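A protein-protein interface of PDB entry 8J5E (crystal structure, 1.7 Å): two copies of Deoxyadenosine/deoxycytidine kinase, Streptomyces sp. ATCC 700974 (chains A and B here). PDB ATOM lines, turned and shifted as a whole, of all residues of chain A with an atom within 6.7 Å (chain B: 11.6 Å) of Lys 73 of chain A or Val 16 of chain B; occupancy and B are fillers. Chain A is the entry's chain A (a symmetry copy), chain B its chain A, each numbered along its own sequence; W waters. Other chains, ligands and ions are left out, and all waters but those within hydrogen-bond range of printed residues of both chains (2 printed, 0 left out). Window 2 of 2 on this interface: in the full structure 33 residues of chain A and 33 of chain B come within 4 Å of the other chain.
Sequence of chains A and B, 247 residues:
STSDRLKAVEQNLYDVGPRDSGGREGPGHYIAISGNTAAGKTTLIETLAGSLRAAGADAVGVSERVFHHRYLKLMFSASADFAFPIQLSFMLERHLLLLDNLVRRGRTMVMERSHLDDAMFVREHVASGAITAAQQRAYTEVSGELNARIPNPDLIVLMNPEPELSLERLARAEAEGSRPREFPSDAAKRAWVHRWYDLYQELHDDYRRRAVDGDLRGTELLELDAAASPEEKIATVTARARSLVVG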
ATOM      1  N   HIS A  69       8.153  14.455 -13.976  1.00  0.00           N
ATOM      2  CA  HIS A  69       6.726  14.696 -14.042  1.00  0.00           C
ATOM      3  C   HIS A  69       6.439  15.790 -15.063  1.00  0.00           C
ATOM      4  O   HIS A  69       7.267  16.672 -15.321  1.00  0.00           O
ATOM      5  CB  HIS A  69       6.181  15.085 -12.661  1.00  0.00           C
ATOM      6  CG  HIS A  69       4.717  14.828 -12.510  1.00  0.00           C
ATOM      7  ND1 HIS A  69       3.761  15.744 -12.902  1.00  0.00           N
ATOM      8  CD2 HIS A  69       4.039  13.739 -12.073  1.00  0.00           C
ATOM      9  CE1 HIS A  69       2.558  15.235 -12.690  1.00  0.00           C
ATOM     10  NE2 HIS A  69       2.697  14.020 -12.188  1.00  0.00           N
ATOM     11  N   ARG A  70       5.250  15.723 -15.655  1.00  0.00           N
ATOM     12  CA  ARG A  70       4.822  16.806 -16.519  1.00  0.00           C
ATOM     13  C   ARG A  70       4.847  18.157 -15.813  1.00  0.00           C
ATOM     14  O   ARG A  70       5.009  19.183 -16.480  1.00  0.00           O
ATOM     15  CB  ARG A  70       3.442  16.477 -17.069  1.00  0.00           C
ATOM     16  CG  ARG A  70       3.553  15.439 -18.166  1.00  0.00           C
ATOM     17  CD  ARG A  70       2.223  15.001 -18.714  1.00  0.00           C
ATOM     18  NE  ARG A  70       1.590  14.030 -17.834  1.00  0.00           N
ATOM     19  CZ  ARG A  70       0.518  13.322 -18.156  1.00  0.00           C
ATOM     20  NH1 ARG A  70      -0.061  13.449 -19.339  1.00  0.00           N
ATOM     21  NH2 ARG A  70       0.019  12.462 -17.272  1.00  0.00           N
ATOM     22  N   TYR A  71       4.736  18.180 -14.488  1.00  0.00           N
ATOM     23  CA  TYR A  71       4.760  19.420 -13.726  1.00  0.00           C
ATOM     24  C   TYR A  71       6.163  19.806 -13.238  1.00  0.00           C
ATOM     25  O   TYR A  71       6.278  20.706 -12.395  1.00  0.00           O
ATOM     26  CB  TYR A  71       3.811  19.323 -12.520  1.00  0.00           C
ATOM     27  CG  TYR A  71       2.323  19.297 -12.856  1.00  0.00           C
ATOM     28  CD1 TYR A  71       1.765  20.210 -13.745  1.00  0.00           C
ATOM     29  CD2 TYR A  71       1.483  18.350 -12.282  1.00  0.00           C
ATOM     30  CE1 TYR A  71       0.412  20.172 -14.051  1.00  0.00           C
ATOM     31  CE2 TYR A  71       0.127  18.300 -12.587  1.00  0.00           C
ATOM     32  CZ  TYR A  71      -0.403  19.214 -13.467  1.00  0.00           C
ATOM     33  OH  TYR A  71      -1.750  19.177 -13.766  1.00  0.00           O
ATOM     34  N   LEU A  72       7.220  19.178 -13.770  1.00  0.00           N
ATOM     35  CA  LEU A  72       8.578  19.349 -13.239  1.00  0.00           C
ATOM     36  C   LEU A  72       8.969  20.815 -13.050  1.00  0.00           C
ATOM     37  O   LEU A  72       9.522  21.187 -12.007  1.00  0.00           O
ATOM     38  CB  LEU A  72       9.596  18.658 -14.156  1.00  0.00           C
ATOM     39  CG  LEU A  72      11.053  18.871 -13.719  1.00  0.00           C
ATOM     40  CD1 LEU A  72      11.257  18.256 -12.359  1.00  0.00           C
ATOM     41  CD2 LEU A  72      12.048  18.271 -14.704  1.00  0.00           C
ATOM     42  N   LYS A  73       8.685  21.670 -14.041  1.00  0.00           N
ATOM     43  CA  LYS A  73       9.129  23.059 -13.949  1.00  0.00           C
ATOM     44  C   LYS A  73       8.598  23.739 -12.694  1.00  0.00           C
ATOM     45  O   LYS A  73       9.276  24.608 -12.128  1.00  0.00           O
ATOM     46  CB  LYS A  73       8.681  23.837 -15.190  1.00  0.00           C
ATOM     47  CG  LYS A  73       9.510  23.602 -16.447  1.00  0.00           C
ATOM     48  CD  LYS A  73       9.120  24.638 -17.519  1.00  0.00           C
ATOM     49  CE  LYS A  73       9.554  24.218 -18.924  1.00  0.00           C
ATOM     50  NZ  LYS A  73      10.070  25.375 -19.730  1.00  0.00           N
ATOM     51  N   LEU A  74       7.403  23.350 -12.234  1.00  0.00           N
ATOM     52  CA  LEU A  74       6.824  24.017 -11.074  1.00  0.00           C
ATOM     53  C   LEU A  74       7.585  23.718  -9.796  1.00  0.00           C
ATOM     54  O   LEU A  74       7.429  24.459  -8.822  1.00  0.00           O
ATOM     55  CB  LEU A  74       5.350  23.631 -10.910  1.00  0.00           C
ATOM     56  CG  LEU A  74       4.466  24.047 -12.090  1.00  0.00           C
ATOM     57  CD1 LEU A  74       3.090  23.441 -11.942  1.00  0.00           C
ATOM     58  CD2 LEU A  74       4.371  25.575 -12.212  1.00  0.00           C
ATOM     59  N   MET A  75       8.428  22.671  -9.772  1.00  0.00           N
ATOM     60  CA  MET A  75       9.131  22.428  -8.519  1.00  0.00           C
ATOM     61  C   MET A  75      10.196  23.504  -8.324  1.00  0.00           C
ATOM     62  O   MET A  75      10.619  23.768  -7.191  1.00  0.00           O
ATOM     63  CB  MET A  75       9.753  21.015  -8.507  1.00  0.00           C
ATOM     64  CG  MET A  75      10.895  20.832  -7.523  1.00  0.00           C
ATOM     65  SD  MET A  75      11.053  19.036  -7.185  1.00  0.00           S
ATOM     66  CE  MET A  75      11.634  18.454  -8.782  1.00  0.00           C
ATOM     67  N   PHE A  76      10.602  24.161  -9.417  1.00  0.00           N
ATOM     68  CA  PHE A  76      11.596  25.225  -9.378  1.00  0.00           C
ATOM     69  C   PHE A  76      11.000  26.618  -9.511  1.00  0.00           C
ATOM     70  O   PHE A  76      11.612  27.575  -9.024  1.00  0.00           O
ATOM     71  CB  PHE A  76      12.646  25.002 -10.473  1.00  0.00           C
ATOM     72  CG  PHE A  76      13.255  23.633 -10.433  1.00  0.00           C
ATOM     73  CD1 PHE A  76      13.965  23.224  -9.315  1.00  0.00           C
ATOM     74  CD2 PHE A  76      13.090  22.738 -11.484  1.00  0.00           C
ATOM     75  CE1 PHE A  76      14.518  21.953  -9.244  1.00  0.00           C
ATOM     76  CE2 PHE A  76      13.643  21.461 -11.423  1.00  0.00           C
ATOM     77  CZ  PHE A  76      14.350  21.070 -10.288  1.00  0.00           C
ATOM     78  N   SER A  77       9.822  26.757 -10.123  1.00  0.00           N
ATOM     79  CA  SER A  77       9.197  28.076 -10.219  1.00  0.00           C
ATOM     80  C   SER A  77       8.138  28.317  -9.154  1.00  0.00           C
ATOM     81  O   SER A  77       7.780  29.476  -8.907  1.00  0.00           O
ATOM     82  CB  SER A  77       8.567  28.268 -11.603  1.00  0.00           C
ATOM     83  OG  SER A  77       7.429  27.447 -11.741  1.00  0.00           O
ATOM     84  N   ALA A  78       7.620  27.257  -8.539  1.00  0.00           N
ATOM     85  CA  ALA A  78       6.605  27.336  -7.491  1.00  0.00           C
ATOM     86  C   ALA A  78       6.950  26.334  -6.394  1.00  0.00           C
ATOM     87  O   ALA A  78       6.112  25.547  -5.953  1.00  0.00           O
ATOM     88  CB  ALA A  78       5.212  27.083  -8.059  1.00  0.00           C
ATOM     89  N   SER A  79       8.211  26.381  -5.950  1.00  0.00           N
ATOM     90  CA  SER A  79       8.778  25.340  -5.093  1.00  0.00           C
ATOM     91  C   SER A  79       7.990  25.156  -3.802  1.00  0.00           C
ATOM     92  O   SER A  79       7.799  24.024  -3.343  1.00  0.00           O
ATOM     93  CB  SER A  79      10.233  25.690  -4.775  1.00  0.00           C
ATOM     94  OG  SER A  79      10.879  26.210  -5.938  1.00  0.00           O
ATOM     95  N   PHE A  82       5.019  22.991  -4.964  1.00  0.00           N
ATOM     96  CA  PHE A  82       5.132  21.780  -5.765  1.00  0.00           C
ATOM     97  C   PHE A  82       6.332  20.909  -5.440  1.00  0.00           C
ATOM     98  O   PHE A  82       6.386  19.770  -5.922  1.00  0.00           O
ATOM     99  CB  PHE A  82       5.161  22.136  -7.258  1.00  0.00           C
ATOM    100  CG  PHE A  82       3.804  22.452  -7.796  1.00  0.00           C
ATOM    101  CD1 PHE A  82       3.257  23.714  -7.610  1.00  0.00           C
ATOM    102  CD2 PHE A  82       3.037  21.474  -8.405  1.00  0.00           C
ATOM    103  CE1 PHE A  82       1.989  24.003  -8.063  1.00  0.00           C
ATOM    104  CE2 PHE A  82       1.756  21.762  -8.857  1.00  0.00           C
ATOM    105  CZ  PHE A  82       1.241  23.022  -8.681  1.00  0.00           C
ATOM    106  N   PRO A 180      14.094  21.618 -22.352  1.00  0.00           N
ATOM    107  CA  PRO A 180      13.465  22.890 -21.991  1.00  0.00           C
ATOM    108  C   PRO A 180      14.233  23.559 -20.868  1.00  0.00           C
ATOM    109  O   PRO A 180      14.954  22.911 -20.104  1.00  0.00           O
ATOM    110  CB  PRO A 180      12.057  22.489 -21.526  1.00  0.00           C
ATOM    111  CG  PRO A 180      11.937  21.036 -21.745  1.00  0.00           C
ATOM    112  CD  PRO A 180      13.298  20.460 -21.922  1.00  0.00           C
ATOM    113  N   ARG A 181      14.067  24.878 -20.777  1.00  0.00           N
ATOM    114  CA  ARG A 181      14.572  25.643 -19.636  1.00  0.00           C
ATOM    115  C   ARG A 181      13.677  25.340 -18.450  1.00  0.00           C
ATOM    116  O   ARG A 181      12.549  25.828 -18.374  1.00  0.00           O
ATOM    117  CB  ARG A 181      14.562  27.137 -19.931  1.00  0.00           C
ATOM    118  CG  ARG A 181      15.288  27.522 -21.194  1.00  0.00           C
ATOM    119  CD  ARG A 181      16.045  28.820 -21.021  1.00  0.00           C
ATOM    120  NE  ARG A 181      16.722  29.181 -22.259  1.00  0.00           N
ATOM    121  CZ  ARG A 181      18.040  29.229 -22.401  1.00  0.00           C
ATOM    122  NH1 ARG A 181      18.854  28.943 -21.396  1.00  0.00           N
ATOM    123  NH2 ARG A 181      18.554  29.551 -23.587  1.00  0.00           N
ATOM    124  N   GLU A 182      14.156  24.532 -17.522  1.00  0.00           N
ATOM    125  CA  GLU A 182      13.272  24.101 -16.453  1.00  0.00           C
ATOM    126  C   GLU A 182      13.384  24.964 -15.203  1.00  0.00           C
ATOM    127  O   GLU A 182      12.631  24.749 -14.249  1.00  0.00           O
ATOM    128  CB  GLU A 182      13.522  22.629 -16.151  1.00  0.00           C
ATOM    129  CG  GLU A 182      12.615  21.799 -17.057  1.00  0.00           C
ATOM    130  CD  GLU A 182      13.114  20.409 -17.347  1.00  0.00           C
ATOM    131  OE1 GLU A 182      14.248  20.062 -16.944  1.00  0.00           O
ATOM    132  OE2 GLU A 182      12.349  19.667 -17.997  1.00  0.00           O
ATOM    133  N   PHE A 183      14.266  25.953 -15.202  1.00  0.00           N
ATOM    134  CA  PHE A 183      14.439  26.823 -14.053  1.00  0.00           C
ATOM    135  C   PHE A 183      13.888  28.214 -14.340  1.00  0.00           C
ATOM    136  O   PHE A 183      13.789  28.630 -15.501  1.00  0.00           O
ATOM    137  CB  PHE A 183      15.928  26.902 -13.676  1.00  0.00           C
ATOM    138  CG  PHE A 183      16.500  25.576 -13.250  1.00  0.00           C
ATOM    139  CD1 PHE A 183      16.316  25.117 -11.953  1.00  0.00           C
ATOM    140  CD2 PHE A 183      17.196  24.776 -14.152  1.00  0.00           C
ATOM    141  CE1 PHE A 183      16.819  23.886 -11.561  1.00  0.00           C
ATOM    142  CE2 PHE A 183      17.703  23.546 -13.762  1.00  0.00           C
ATOM    143  CZ  PHE A 183      17.512  23.102 -12.464  1.00  0.00           C
ATOM    144  N   PRO A 184      13.517  28.967 -13.300  1.00  0.00           N
ATOM    145  CA  PRO A 184      12.845  30.261 -13.518  1.00  0.00           C
ATOM    146  C   PRO A 184      13.787  31.418 -13.806  1.00  0.00           C
ATOM    147  O   PRO A 184      13.303  32.507 -14.149  1.00  0.00           O
ATOM    148  CB  PRO A 184      12.100  30.495 -12.198  1.00  0.00           C
ATOM    149  CG  PRO A 184      12.884  29.751 -11.183  1.00  0.00           C
ATOM    150  CD  PRO A 184      13.492  28.557 -11.883  1.00  0.00           C
ATOM    151  N   GLN B  11      -7.694  19.206 -23.034  1.00  0.00           N
ATOM    152  CA  GLN B  11      -8.204  19.887 -21.854  1.00  0.00           C
ATOM    153  C   GLN B  11      -7.134  20.703 -21.142  1.00  0.00           C
ATOM    154  O   GLN B  11      -7.429  21.306 -20.104  1.00  0.00           O
ATOM    155  CB  GLN B  11      -8.820  18.865 -20.894  1.00  0.00           C
ATOM    156  CG  GLN B  11     -10.204  18.413 -21.321  1.00  0.00           C
ATOM    157  CD  GLN B  11     -10.995  17.823 -20.175  1.00  0.00           C
ATOM    158  OE1 GLN B  11     -12.066  18.327 -19.818  1.00  0.00           O
ATOM    159  NE2 GLN B  11     -10.483  16.733 -19.599  1.00  0.00           N
ATOM    160  N   ASN B  12      -5.905  20.729 -21.669  1.00  0.00           N
ATOM    161  CA  ASN B  12      -4.814  21.530 -21.109  1.00  0.00           C
ATOM    162  C   ASN B  12      -4.584  21.232 -19.631  1.00  0.00           C
ATOM    163  O   ASN B  12      -4.337  22.133 -18.830  1.00  0.00           O
ATOM    164  CB  ASN B  12      -5.058  23.023 -21.312  1.00  0.00           C
ATOM    165  CG  ASN B  12      -3.775  23.828 -21.242  1.00  0.00           C
ATOM    166  OD1 ASN B  12      -2.694  23.322 -21.549  1.00  0.00           O
ATOM    167  ND2 ASN B  12      -3.885  25.075 -20.808  1.00  0.00           N
ATOM    168  N   LEU B  13      -4.641  19.950 -19.268  1.00  0.00           N
ATOM    169  CA  LEU B  13      -4.500  19.581 -17.865  1.00  0.00           C
ATOM    170  C   LEU B  13      -3.077  19.750 -17.351  1.00  0.00           C
ATOM    171  O   LEU B  13      -2.878  19.858 -16.134  1.00  0.00           O
ATOM    172  CB  LEU B  13      -4.957  18.137 -17.660  1.00  0.00           C
ATOM    173  CG  LEU B  13      -6.463  17.878 -17.774  1.00  0.00           C
ATOM    174  CD1 LEU B  13      -6.763  16.401 -17.566  1.00  0.00           C
ATOM    175  CD2 LEU B  13      -7.224  18.740 -16.782  1.00  0.00           C
ATOM    176  N   TYR B  14      -2.078  19.790 -18.233  1.00  0.00           N
ATOM    177  CA  TYR B  14      -0.716  19.796 -17.708  1.00  0.00           C
ATOM    178  C   TYR B  14       0.080  21.009 -18.197  1.00  0.00           C
ATOM    179  O   TYR B  14       1.200  20.866 -18.693  1.00  0.00           O
ATOM    180  CB  TYR B  14      -0.010  18.474 -18.063  1.00  0.00           C
ATOM    181  CG  TYR B  14      -0.595  17.313 -17.280  1.00  0.00           C
ATOM    182  CD1 TYR B  14      -0.093  16.967 -16.036  1.00  0.00           C
ATOM    183  CD2 TYR B  14      -1.605  16.517 -17.821  1.00  0.00           C
ATOM    184  CE1 TYR B  14      -0.634  15.908 -15.309  1.00  0.00           C
ATOM    185  CE2 TYR B  14      -2.140  15.447 -17.109  1.00  0.00           C
ATOM    186  CZ  TYR B  14      -1.649  15.147 -15.855  1.00  0.00           C
ATOM    187  OH  TYR B  14      -2.167  14.085 -15.135  1.00  0.00           O
ATOM    188  N   ASP B  15      -0.473  22.209 -18.024  1.00  0.00           N
ATOM    189  CA  ASP B  15       0.137  23.445 -18.504  1.00  0.00           C
ATOM    190  C   ASP B  15       0.901  24.095 -17.350  1.00  0.00           C
ATOM    191  O   ASP B  15       0.292  24.529 -16.367  1.00  0.00           O
ATOM    192  CB  ASP B  15      -0.949  24.377 -19.055  1.00  0.00           C
ATOM    193  CG  ASP B  15      -0.440  25.779 -19.409  1.00  0.00           C
ATOM    194  OD1 ASP B  15       0.762  26.088 -19.247  1.00  0.00           O
ATOM    195  OD2 ASP B  15      -1.277  26.594 -19.854  1.00  0.00           O
ATOM    196  N   VAL B  16       2.231  24.177 -17.472  1.00  0.00           N
ATOM    197  CA  VAL B  16       3.063  24.743 -16.409  1.00  0.00           C
ATOM    198  C   VAL B  16       3.309  26.237 -16.609  1.00  0.00           C
ATOM    199  O   VAL B  16       4.099  26.834 -15.867  1.00  0.00           O
ATOM    200  CB  VAL B  16       4.402  23.997 -16.267  1.00  0.00           C
ATOM    201  CG1 VAL B  16       4.173  22.552 -15.835  1.00  0.00           C
ATOM    202  CG2 VAL B  16       5.215  24.066 -17.555  1.00  0.00           C
ATOM    203  N   GLY B  17       2.668  26.855 -17.606  1.00  0.00           N
ATOM    204  CA  GLY B  17       2.799  28.269 -17.806  1.00  0.00           C
ATOM    205  C   GLY B  17       2.086  29.053 -16.719  1.00  0.00           C
ATOM    206  O   GLY B  17       1.420  28.484 -15.842  1.00  0.00           O
ATOM    207  N   PRO B  18       2.216  30.378 -16.769  1.00  0.00           N
ATOM    208  CA  PRO B  18       1.559  31.221 -15.763  1.00  0.00           C
ATOM    209  C   PRO B  18       0.041  31.149 -15.860  1.00  0.00           C
ATOM    210  O   PRO B  18      -0.535  30.812 -16.898  1.00  0.00           O
ATOM    211  CB  PRO B  18       2.073  32.628 -16.093  1.00  0.00           C
ATOM    212  CG  PRO B  18       2.384  32.562 -17.564  1.00  0.00           C
ATOM    213  CD  PRO B  18       2.979  31.183 -17.740  1.00  0.00           C
ATOM    214  N   ARG B  19      -0.607  31.462 -14.737  1.00  0.00           N
ATOM    215  CA  ARG B  19      -2.063  31.521 -14.706  1.00  0.00           C
ATOM    216  C   ARG B  19      -2.570  32.521 -15.739  1.00  0.00           C
ATOM    217  O   ARG B  19      -2.009  33.608 -15.903  1.00  0.00           O
ATOM    218  CB  ARG B  19      -2.558  31.908 -13.306  1.00  0.00           C
ATOM    219  CG  ARG B  19      -4.083  31.963 -13.196  1.00  0.00           C
ATOM    220  CD  ARG B  19      -4.585  32.811 -12.020  1.00  0.00           C
ATOM    221  NE  ARG B  19      -4.705  32.033 -10.794  1.00  0.00           N
ATOM    222  CZ  ARG B  19      -5.836  31.839 -10.127  1.00  0.00           C
ATOM    223  NH1 ARG B  19      -6.979  32.373 -10.528  1.00  0.00           N
ATOM    224  NH2 ARG B  19      -5.821  31.081  -9.035  1.00  0.00           N
ATOM    225  N   ASP B  20      -3.625  32.134 -16.457  1.00  0.00           N
ATOM    226  CA  ASP B  20      -4.225  32.991 -17.471  1.00  0.00           C
ATOM    227  C   ASP B  20      -5.676  33.290 -17.111  1.00  0.00           C
ATOM    228  O   ASP B  20      -6.594  32.981 -17.879  1.00  0.00           O
ATOM    229  CB  ASP B  20      -4.138  32.339 -18.853  1.00  0.00           C
ATOM    230  N   LEU B  96      -1.691  16.411  -7.549  1.00  0.00           N
ATOM    231  CA  LEU B  96      -0.982  17.344  -8.425  1.00  0.00           C
ATOM    232  C   LEU B  96      -1.921  17.956  -9.451  1.00  0.00           C
ATOM    233  O   LEU B  96      -1.813  19.147  -9.765  1.00  0.00           O
ATOM    234  CB  LEU B  96       0.170  16.629  -9.131  1.00  0.00           C
ATOM    235  CG  LEU B  96       1.433  16.473  -8.284  1.00  0.00           C
ATOM    236  CD1 LEU B  96       2.344  15.429  -8.870  1.00  0.00           C
ATOM    237  CD2 LEU B  96       2.143  17.820  -8.233  1.00  0.00           C
ATOM    238  N   LEU B  97      -2.847  17.148  -9.991  1.00  0.00           N
ATOM    239  CA  LEU B  97      -3.816  17.680 -10.949  1.00  0.00           C
ATOM    240  C   LEU B  97      -4.655  18.785 -10.321  1.00  0.00           C
ATOM    241  O   LEU B  97      -4.888  19.826 -10.951  1.00  0.00           O
ATOM    242  CB  LEU B  97      -4.723  16.563 -11.486  1.00  0.00           C
ATOM    243  CG  LEU B  97      -5.298  16.771 -12.898  1.00  0.00           C
ATOM    244  CD1 LEU B  97      -4.200  17.033 -13.924  1.00  0.00           C
ATOM    245  CD2 LEU B  97      -6.230  15.675 -13.384  1.00  0.00           C
ATOM    246  N   LEU B  99      -3.862  20.538  -7.514  1.00  0.00           N
ATOM    247  CA  LEU B  99      -3.018  21.635  -7.063  1.00  0.00           C
ATOM    248  C   LEU B  99      -2.698  22.581  -8.213  1.00  0.00           C
ATOM    249  O   LEU B  99      -2.642  23.806  -8.025  1.00  0.00           O
ATOM    250  CB  LEU B  99      -1.730  21.087  -6.446  1.00  0.00           C
ATOM    251  CG  LEU B  99      -0.826  22.100  -5.737  1.00  0.00           C
ATOM    252  CD1 LEU B  99      -1.490  22.717  -4.508  1.00  0.00           C
ATOM    253  CD2 LEU B  99       0.506  21.411  -5.354  1.00  0.00           C
ATOM    254  N   ASP B 100      -2.491  22.034  -9.412  1.00  0.00           N
ATOM    255  CA  ASP B 100      -2.205  22.878 -10.571  1.00  0.00           C
ATOM    256  C   ASP B 100      -3.472  23.486 -11.167  1.00  0.00           C
ATOM    257  O   ASP B 100      -3.571  24.708 -11.323  1.00  0.00           O
ATOM    258  CB  ASP B 100      -1.467  22.085 -11.650  1.00  0.00           C
ATOM    259  CG  ASP B 100      -1.275  22.900 -12.919  1.00  0.00           C
ATOM    260  OD1 ASP B 100      -0.666  23.983 -12.834  1.00  0.00           O
ATOM    261  OD2 ASP B 100      -1.758  22.477 -13.984  1.00  0.00           O
ATOM    262  N   ASN B 101      -4.444  22.648 -11.528  1.00  0.00           N
ATOM    263  CA  ASN B 101      -5.592  23.156 -12.282  1.00  0.00           C
ATOM    264  C   ASN B 101      -6.544  23.956 -11.402  1.00  0.00           C
ATOM    265  O   ASN B 101      -7.022  25.027 -11.802  1.00  0.00           O
ATOM    266  CB  ASN B 101      -6.342  22.004 -12.937  1.00  0.00           C
ATOM    267  CG  ASN B 101      -5.623  21.462 -14.134  1.00  0.00           C
ATOM    268  OD1 ASN B 101      -5.777  21.971 -15.243  1.00  0.00           O
ATOM    269  ND2 ASN B 101      -4.810  20.436 -13.922  1.00  0.00           N
ATOM    270  N   ARG B 104      -3.706  26.492  -8.452  1.00  0.00           N
ATOM    271  CA  ARG B 104      -2.772  27.418  -9.095  1.00  0.00           C
ATOM    272  C   ARG B 104      -3.417  28.166 -10.257  1.00  0.00           C
ATOM    273  O   ARG B 104      -3.208  29.377 -10.410  1.00  0.00           O
ATOM    274  CB  ARG B 104      -1.529  26.674  -9.578  1.00  0.00           C
ATOM    275  CG  ARG B 104      -0.405  27.610 -10.037  1.00  0.00           C
ATOM    276  CD  ARG B 104       0.802  26.828 -10.520  1.00  0.00           C
ATOM    277  NE  ARG B 104       0.590  26.277 -11.850  1.00  0.00           N
ATOM    278  CZ  ARG B 104       0.937  26.897 -12.970  1.00  0.00           C
ATOM    279  NH1 ARG B 104       1.497  28.095 -12.944  1.00  0.00           N
ATOM    280  NH2 ARG B 104       0.707  26.307 -14.139  1.00  0.00           N
ATOM    281  N   ARG B 105      -4.183  27.470 -11.098  1.00  0.00           N
ATOM    282  CA  ARG B 105      -4.716  28.076 -12.317  1.00  0.00           C
ATOM    283  C   ARG B 105      -6.176  28.496 -12.198  1.00  0.00           C
ATOM    284  O   ARG B 105      -6.708  29.098 -13.140  1.00  0.00           O
ATOM    285  CB  ARG B 105      -4.535  27.126 -13.499  1.00  0.00           C
ATOM    286  CG  ARG B 105      -3.083  26.914 -13.834  1.00  0.00           C
ATOM    287  CD  ARG B 105      -2.941  26.480 -15.254  1.00  0.00           C
ATOM    288  NE  ARG B 105      -2.834  25.031 -15.322  1.00  0.00           N
ATOM    289  CZ  ARG B 105      -3.342  24.279 -16.287  1.00  0.00           C
ATOM    290  NH1 ARG B 105      -4.030  24.805 -17.291  1.00  0.00           N
ATOM    291  NH2 ARG B 105      -3.144  22.966 -16.248  1.00  0.00           N
ATOM    292  N   ARG B 107      -9.049  26.892 -12.269  1.00  0.00           N
ATOM    293  CA  ARG B 107     -10.014  26.303 -13.183  1.00  0.00           C
ATOM    294  C   ARG B 107     -11.094  25.568 -12.404  1.00  0.00           C
ATOM    295  O   ARG B 107     -10.979  25.337 -11.197  1.00  0.00           O
ATOM    296  CB  ARG B 107      -9.322  25.366 -14.174  1.00  0.00           C
ATOM    297  CG  ARG B 107      -8.083  25.988 -14.815  1.00  0.00           C
ATOM    298  CD  ARG B 107      -7.433  25.019 -15.795  1.00  0.00           C
ATOM    299  NE  ARG B 107      -8.211  24.877 -17.020  1.00  0.00           N
ATOM    300  CZ  ARG B 107      -8.080  23.874 -17.873  1.00  0.00           C
ATOM    301  NH1 ARG B 107      -7.240  22.874 -17.643  1.00  0.00           N
ATOM    302  NH2 ARG B 107      -8.805  23.874 -18.992  1.00  0.00           N
HETATM  303  O   HOH W   1       3.990  19.849 -18.861  1.00  0.00           O
HETATM  304  O   HOH W   2       6.877  27.070 -14.235  1.00  0.00           O
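The backbone carbonyl oxygen of Leu 99 of chain B is in hydrogen-bond range of the backbone NH of Arg 104 of chain B, 2.9 Å away.
O of Gly 17 of chain B sits at hydrogen-bond distance from NH2 of Arg 104 of chain B (2.9 Å).
Water W2 lies within hydrogen-bond range of the side-chain hydroxyl (OG) of Ser 77 of chain A (2.6 Å) and the backbone carbonyl oxygen (O) of Val 16 of chain B (3.2 Å).
Water W1 lies within hydrogen-bond range of O of Arg 70 of chain A and O of Tyr 14 of chain B.
Tyr 71 of chain A touches seven residues of chain B.
Leu 72 of chain A touches none of the printed residues of chain B.
Of chain B, only Val 16, Asp 100 and Arg 104 come within 4 Å of Leu 74 of chain A.
No residue of chain B comes within 4 Å of Ser 77 of chain A.
No residue of chain B comes within 4 Å of Ala 78 of chain A.
No residue of chain B comes within 4 Å of Pro 180 of chain A.
Printed residues of chain A within 4 Å of Leu 99 of chain B: Phe 82 (3.7 Å).
Printed residues of chain A within 4 Å of Asp 100 of chain B: Tyr 71 (3.2 Å), Leu 74 (3.9 Å) and Phe 82 (3.9 Å).
The nearest residue of chain B that does not touch Lys 73 of chain A is Gly 17 of chain B (6.8 Å).
The nearest residue of chain A that does not touch Val 16 of chain B is Leu 72 of chain A (5.0 Å).
Printed residues of chain A that touch a printed residue of chain B: His 69, Arg 70, Tyr 71, Lys 73, Leu 74 and Phe 82.
Hydrophobic or aromatic side chains of chain A that line the printed part of chain B: His 69, Tyr 71, Leu 74 and Phe 82.
Of the 18 printed residues of chain B, 9 touch a printed residue of chain A.
Hydrophobic or aromatic side chains of chain B that line the printed part of chain A: Tyr 14, Val 16, Leu 96, Leu 97 and Leu 99.
Along chain B the printed residues that touch a printed residue of chain A span positions 13 to 104.
Among the printed residues, no Asp or Glu carboxylate lies within 4 Å of a Lys or Arg side-chain nitrogen of the other chain.
CA of Tyr 71 of chain A touches CG1 of Val 16 of chain B, at 3.8 Å.
Leu 97 of chain B touches Tyr 71 of chain A.
CG2 of Val 16 of chain B touches CD of Lys 73 of chain A (3.9 Å).
Leu 74 of chain A touches Val 16 of chain B.
CD1 of Leu 74 of chain A touches OD1 of Asp 100 of chain B, 3.9 Å away.
The side-chain hydroxyl of Tyr 71 of chain A sits close to the side-chain carboxylate of Asp 100 of chain B (3.3 Å).
The side-chain hydroxyl (OH) of Tyr 71 of chain A sits at hydrogen-bond distance from the side-chain amide nitrogen (ND2) of Asn 101 of chain B, at 3.3 Å.
The side-chain hydroxyl of Tyr 14 of chain B sits at hydrogen-bond distance from the guanidinium group of Arg 70 of chain A (3.5 Å).
The backbone carbonyl oxygen of Leu 13 of chain B lies within hydrogen-bond range of the side-chain hydroxyl of Tyr 71 of chain A (2.7 Å).
No position is printed for both chains.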
